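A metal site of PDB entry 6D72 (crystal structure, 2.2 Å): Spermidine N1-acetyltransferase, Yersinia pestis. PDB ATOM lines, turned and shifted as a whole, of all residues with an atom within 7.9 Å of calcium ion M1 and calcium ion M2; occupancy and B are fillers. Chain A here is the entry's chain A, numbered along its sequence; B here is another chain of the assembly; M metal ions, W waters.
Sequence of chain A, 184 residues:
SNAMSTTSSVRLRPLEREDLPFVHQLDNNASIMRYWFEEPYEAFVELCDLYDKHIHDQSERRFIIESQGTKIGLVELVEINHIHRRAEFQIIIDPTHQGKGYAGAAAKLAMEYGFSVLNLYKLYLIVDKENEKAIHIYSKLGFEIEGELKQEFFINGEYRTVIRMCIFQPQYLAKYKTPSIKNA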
ATOM      1  N   PHE A  37     -25.442 -14.396  18.410  1.00  0.00           N
ATOM      2  CA  PHE A  37     -24.150 -13.870  17.992  1.00  0.00           C
ATOM      3  C   PHE A  37     -23.148 -14.994  17.874  1.00  0.00           C
ATOM      4  O   PHE A  37     -22.044 -14.880  18.386  1.00  0.00           O
ATOM      5  CB  PHE A  37     -23.685 -12.752  18.938  1.00  0.00           C
ATOM      6  CG  PHE A  37     -24.474 -11.467  18.748  1.00  0.00           C
ATOM      7  CD1 PHE A  37     -25.705 -11.279  19.370  1.00  0.00           C
ATOM      8  CD2 PHE A  37     -23.970 -10.441  17.969  1.00  0.00           C
ATOM      9  CE1 PHE A  37     -26.436 -10.105  19.205  1.00  0.00           C
ATOM     10  CE2 PHE A  37     -24.691  -9.281  17.768  1.00  0.00           C
ATOM     11  CZ  PHE A  37     -25.940  -9.105  18.403  1.00  0.00           C
ATOM     12  N   GLU A  38     -23.579 -16.079  17.252  1.00  0.00           N
ATOM     13  CA  GLU A  38     -22.771 -17.221  16.902  1.00  0.00           C
ATOM     14  C   GLU A  38     -22.347 -18.063  18.089  1.00  0.00           C
ATOM     15  O   GLU A  38     -21.516 -18.917  17.946  1.00  0.00           O
ATOM     16  CB  GLU A  38     -21.568 -16.792  16.015  1.00  0.00           C
ATOM     17  CG  GLU A  38     -22.015 -15.861  14.851  1.00  0.00           C
ATOM     18  CD  GLU A  38     -20.899 -15.595  13.821  1.00  0.00           C
ATOM     19  OE1 GLU A  38     -21.012 -14.654  13.006  1.00  0.00           O
ATOM     20  OE2 GLU A  38     -19.883 -16.331  13.868  1.00  0.00           O
ATOM     21  N   SER A  59     -22.779  -6.665  14.769  1.00  0.00           N
ATOM     22  CA  SER A  59     -22.702  -7.684  13.746  1.00  0.00           C
ATOM     23  C   SER A  59     -24.028  -8.450  13.502  1.00  0.00           C
ATOM     24  O   SER A  59     -24.158  -9.164  12.503  1.00  0.00           O
ATOM     25  CB  SER A  59     -21.580  -8.672  14.095  1.00  0.00           C
ATOM     26  OG  SER A  59     -21.957  -9.486  15.185  1.00  0.00           O
ATOM     27  N   GLU A  60     -25.007  -8.307  14.412  1.00  0.00           N
ATOM     28  CA  GLU A  60     -26.358  -8.825  14.213  1.00  0.00           C
ATOM     29  C   GLU A  60     -27.350  -7.805  14.753  1.00  0.00           C
ATOM     30  O   GLU A  60     -27.013  -6.992  15.636  1.00  0.00           O
ATOM     31  CB  GLU A  60     -26.572 -10.184  14.927  1.00  0.00           C
ATOM     32  CG  GLU A  60     -25.507 -11.265  14.597  1.00  0.00           C
ATOM     33  CD  GLU A  60     -25.769 -12.647  15.226  1.00  0.00           C
ATOM     34  OE1 GLU A  60     -25.076 -13.569  14.761  1.00  0.00           O
ATOM     35  OE2 GLU A  60     -26.602 -12.798  16.185  1.00  0.00           O
ATOM     36  N   VAL A  78     -27.998 -11.165  10.358  1.00  0.00           N
ATOM     37  CA  VAL A  78     -26.781 -11.674  10.899  1.00  0.00           C
ATOM     38  C   VAL A  78     -25.671 -11.598   9.855  1.00  0.00           C
ATOM     39  O   VAL A  78     -25.922 -11.309   8.680  1.00  0.00           O
ATOM     40  CB  VAL A  78     -26.930 -13.121  11.450  1.00  0.00           C
ATOM     41  CG1 VAL A  78     -27.983 -13.179  12.544  1.00  0.00           C
ATOM     42  CG2 VAL A  78     -27.296 -14.133  10.378  1.00  0.00           C
ATOM     43  N   GLU A  79     -24.440 -11.866  10.289  1.00  0.00           N
ATOM     44  CA  GLU A  79     -23.245 -11.752   9.460  1.00  0.00           C
ATOM     45  C   GLU A  79     -23.169 -10.408   8.773  1.00  0.00           C
ATOM     46  O   GLU A  79     -22.852 -10.348   7.589  1.00  0.00           O
ATOM     47  CB  GLU A  79     -23.256 -12.832   8.356  1.00  0.00           C
ATOM     48  CG  GLU A  79     -23.465 -14.269   8.810  1.00  0.00           C
ATOM     49  CD  GLU A  79     -22.258 -14.820   9.600  1.00  0.00           C
ATOM     50  OE1 GLU A  79     -21.421 -13.970   9.950  1.00  0.00           O
ATOM     51  OE2 GLU A  79     -22.168 -16.050   9.857  1.00  0.00           O
ATOM     52  N   ILE A  80     -23.517  -9.358   9.479  1.00  0.00           N
ATOM     53  CA  ILE A  80     -23.581  -8.045   8.848  1.00  0.00           C
ATOM     54  C   ILE A  80     -22.150  -7.606   8.584  1.00  0.00           C
ATOM     55  O   ILE A  80     -21.345  -7.628   9.467  1.00  0.00           O
ATOM     56  CB  ILE A  80     -24.288  -7.015   9.752  1.00  0.00           C
ATOM     57  CG1 ILE A  80     -25.774  -7.401   9.967  1.00  0.00           C
ATOM     58  CG2 ILE A  80     -24.180  -5.589   9.166  1.00  0.00           C
ATOM     59  CD1 ILE A  80     -26.463  -6.545  11.044  1.00  0.00           C
ATOM     60  N   TYR A 124     -29.170 -11.720   1.609  1.00  0.00           N
ATOM     61  CA  TYR A 124     -29.362 -13.098   1.243  1.00  0.00           C
ATOM     62  C   TYR A 124     -29.983 -13.894   2.387  1.00  0.00           C
ATOM     63  O   TYR A 124     -30.014 -13.432   3.555  1.00  0.00           O
ATOM     64  CB  TYR A 124     -28.051 -13.714   0.771  1.00  0.00           C
ATOM     65  CG  TYR A 124     -26.967 -13.854   1.824  1.00  0.00           C
ATOM     66  CD1 TYR A 124     -26.081 -12.829   2.087  1.00  0.00           C
ATOM     67  CD2 TYR A 124     -26.857 -15.006   2.567  1.00  0.00           C
ATOM     68  CE1 TYR A 124     -25.088 -12.938   3.046  1.00  0.00           C
ATOM     69  CE2 TYR A 124     -25.870 -15.147   3.543  1.00  0.00           C
ATOM     70  CZ  TYR A 124     -24.981 -14.139   3.781  1.00  0.00           C
ATOM     71  OH  TYR A 124     -24.026 -14.242   4.784  1.00  0.00           O
ATOM     72  N   PHE B  37     -10.629 -14.052  13.856  1.00  0.00           N
ATOM     73  CA  PHE B  37     -11.839 -14.477  14.545  1.00  0.00           C
ATOM     74  C   PHE B  37     -12.965 -13.494  14.291  1.00  0.00           C
ATOM     75  O   PHE B  37     -13.624 -13.080  15.211  1.00  0.00           O
ATOM     76  CB  PHE B  37     -11.567 -14.700  16.033  1.00  0.00           C
ATOM     77  CG  PHE B  37     -10.756 -15.948  16.297  1.00  0.00           C
ATOM     78  CD1 PHE B  37      -9.395 -15.940  16.205  1.00  0.00           C
ATOM     79  CD2 PHE B  37     -11.393 -17.139  16.670  1.00  0.00           C
ATOM     80  CE1 PHE B  37      -8.631 -17.100  16.447  1.00  0.00           C
ATOM     81  CE2 PHE B  37     -10.641 -18.307  16.904  1.00  0.00           C
ATOM     82  CZ  PHE B  37      -9.260 -18.280  16.810  1.00  0.00           C
ATOM     83  N   GLU B  38     -13.084 -13.086  13.026  1.00  0.00           N
ATOM     84  CA  GLU B  38     -14.170 -12.268  12.527  1.00  0.00           C
ATOM     85  C   GLU B  38     -14.096 -10.816  12.985  1.00  0.00           C
ATOM     86  O   GLU B  38     -15.054 -10.083  12.814  1.00  0.00           O
ATOM     87  CB  GLU B  38     -15.571 -12.925  12.867  1.00  0.00           C
ATOM     88  CG  GLU B  38     -15.578 -14.415  12.426  1.00  0.00           C
ATOM     89  CD  GLU B  38     -16.958 -15.068  12.379  1.00  0.00           C
ATOM     90  OE1 GLU B  38     -17.071 -16.315  12.343  1.00  0.00           O
ATOM     91  OE2 GLU B  38     -17.939 -14.322  12.376  1.00  0.00           O
ATOM     92  N   SER B  59     -13.259 -21.796  17.506  1.00  0.00           N
ATOM     93  CA  SER B  59     -14.015 -21.587  16.285  1.00  0.00           C
ATOM     94  C   SER B  59     -13.167 -21.396  15.022  1.00  0.00           C
ATOM     95  O   SER B  59     -13.675 -21.477  13.916  1.00  0.00           O
ATOM     96  CB  SER B  59     -14.986 -20.406  16.468  1.00  0.00           C
ATOM     97  OG  SER B  59     -14.270 -19.202  16.466  1.00  0.00           O
ATOM     98  N   GLU B  60     -11.860 -21.135  15.195  1.00  0.00           N
ATOM     99  CA  GLU B  60     -10.902 -21.071  14.099  1.00  0.00           C
ATOM    100  C   GLU B  60      -9.605 -21.745  14.563  1.00  0.00           C
ATOM    101  O   GLU B  60      -9.331 -21.797  15.765  1.00  0.00           O
ATOM    102  CB  GLU B  60     -10.644 -19.635  13.630  1.00  0.00           C
ATOM    103  CG  GLU B  60     -11.888 -18.794  13.299  1.00  0.00           C
ATOM    104  CD  GLU B  60     -11.630 -17.391  12.728  1.00  0.00           C
ATOM    105  OE1 GLU B  60     -12.594 -16.789  12.194  1.00  0.00           O
ATOM    106  OE2 GLU B  60     -10.484 -16.845  12.834  1.00  0.00           O
ATOM    107  N   VAL B  78     -11.853 -21.870   9.467  1.00  0.00           N
ATOM    108  CA  VAL B  78     -12.722 -20.947  10.112  1.00  0.00           C
ATOM    109  C   VAL B  78     -14.170 -21.449  10.040  1.00  0.00           C
ATOM    110  O   VAL B  78     -14.474 -22.429   9.348  1.00  0.00           O
ATOM    111  CB  VAL B  78     -12.600 -19.508   9.503  1.00  0.00           C
ATOM    112  CG1 VAL B  78     -11.158 -18.984   9.624  1.00  0.00           C
ATOM    113  CG2 VAL B  78     -13.033 -19.432   8.045  1.00  0.00           C
ATOM    114  N   GLU B  79     -15.043 -20.758  10.790  1.00  0.00           N
ATOM    115  CA  GLU B  79     -16.460 -21.144  10.921  1.00  0.00           C
ATOM    116  C   GLU B  79     -16.587 -22.591  11.339  1.00  0.00           C
ATOM    117  O   GLU B  79     -17.443 -23.297  10.810  1.00  0.00           O
ATOM    118  CB  GLU B  79     -17.211 -20.987   9.583  1.00  0.00           C
ATOM    119  CG  GLU B  79     -17.080 -19.652   8.867  1.00  0.00           C
ATOM    120  CD  GLU B  79     -17.791 -18.528   9.578  1.00  0.00           C
ATOM    121  OE1 GLU B  79     -18.054 -18.726  10.772  1.00  0.00           O
ATOM    122  OE2 GLU B  79     -18.021 -17.451   8.961  1.00  0.00           O
ATOM    123  N   ILE B  80     -15.738 -23.062  12.217  1.00  0.00           N
ATOM    124  CA  ILE B  80     -15.743 -24.467  12.586  1.00  0.00           C
ATOM    125  C   ILE B  80     -16.986 -24.729  13.401  1.00  0.00           C
ATOM    126  O   ILE B  80     -17.220 -24.040  14.333  1.00  0.00           O
ATOM    127  CB  ILE B  80     -14.493 -24.853  13.405  1.00  0.00           C
ATOM    128  CG1 ILE B  80     -13.204 -24.673  12.572  1.00  0.00           C
ATOM    129  CG2 ILE B  80     -14.584 -26.311  13.874  1.00  0.00           C
ATOM    130  CD1 ILE B  80     -11.932 -24.790  13.415  1.00  0.00           C
ATOM    131  N   TYR B 124     -15.311 -26.986   3.116  1.00  0.00           N
ATOM    132  CA  TYR B 124     -15.583 -26.179   1.952  1.00  0.00           C
ATOM    133  C   TYR B 124     -14.637 -24.988   1.879  1.00  0.00           C
ATOM    134  O   TYR B 124     -13.927 -24.662   2.846  1.00  0.00           O
ATOM    135  CB  TYR B 124     -17.043 -25.763   1.931  1.00  0.00           C
ATOM    136  CG  TYR B 124     -17.468 -24.834   3.019  1.00  0.00           C
ATOM    137  CD1 TYR B 124     -17.908 -25.324   4.263  1.00  0.00           C
ATOM    138  CD2 TYR B 124     -17.415 -23.445   2.845  1.00  0.00           C
ATOM    139  CE1 TYR B 124     -18.275 -24.451   5.301  1.00  0.00           C
ATOM    140  CE2 TYR B 124     -17.798 -22.579   3.865  1.00  0.00           C
ATOM    141  CZ  TYR B 124     -18.246 -23.094   5.086  1.00  0.00           C
ATOM    142  OH  TYR B 124     -18.599 -22.245   6.137  1.00  0.00           O
HETATM  143 CA    CA M   1     -19.745 -14.661  11.200  1.00  0.00          CA
HETATM  144 CA    CA M   2     -19.030 -17.260  12.083  1.00  0.00          CA
HETATM  145  O   HOH W   1     -18.386 -13.531   9.607  1.00  0.00           O
HETATM  146  O   HOH W   2     -20.709 -18.943  12.170  1.00  0.00           O
HETATM  147  O   HOH W   3     -17.784 -18.440  13.737  1.00  0.00           O
HETATM  148  O   HOH W   4     -19.890 -12.376  11.861  1.00  0.00           O
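Four residues have an atom within 4 Å of calcium ion M1: Glu 38 of chain A, Glu 79 of chain A, Glu 38 of chain B and Glu 79 of chain B.
OE2 of Glu 38 of chain B binds calcium ion M1 (2.2 Å). Calcium ion M1 is bound by OE1 of Glu 79 of chain A (2.2 Å). OE1 of Glu 38 of chain A binds calcium ion M1, at 2.2 Å. Water W1 binds calcium ion M1 (2.4 Å). Calcium ion M1 is bound by water W4 (2.4 Å). Slightly farther from calcium ion M1 lies OE2 of Glu 79 of chain A (3.1 Å).
N of Glu 79 of chain B sits at hydrogen-bond distance from O of Ser 59 of chain B (3.5 Å).
Calcium ion M2 is bound by OE2 of Glu 38 of chain A. The side-chain carboxylate (OE1) of Glu 38 of chain B binds calcium ion M2. OE1 of Glu 79 of chain B binds calcium ion M2, 2.2 Å away. Water W2 binds calcium ion M2. Calcium ion M2 is bound by water W3, 2.4 Å away. Calcium ion M2 has five donor atoms within binding distance. Slightly farther from calcium ion M2 lies the side-chain carboxylate (OE2) of Glu 38 of chain B (3.1 Å).
Within 4 Å of calcium ion M2: Glu 38 of chain A, Glu 38 of chain B and Glu 79 of chain B. The nearest printed residue that does not touch calcium ion M2 is Glu 79 of chain A (4.03 Å).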
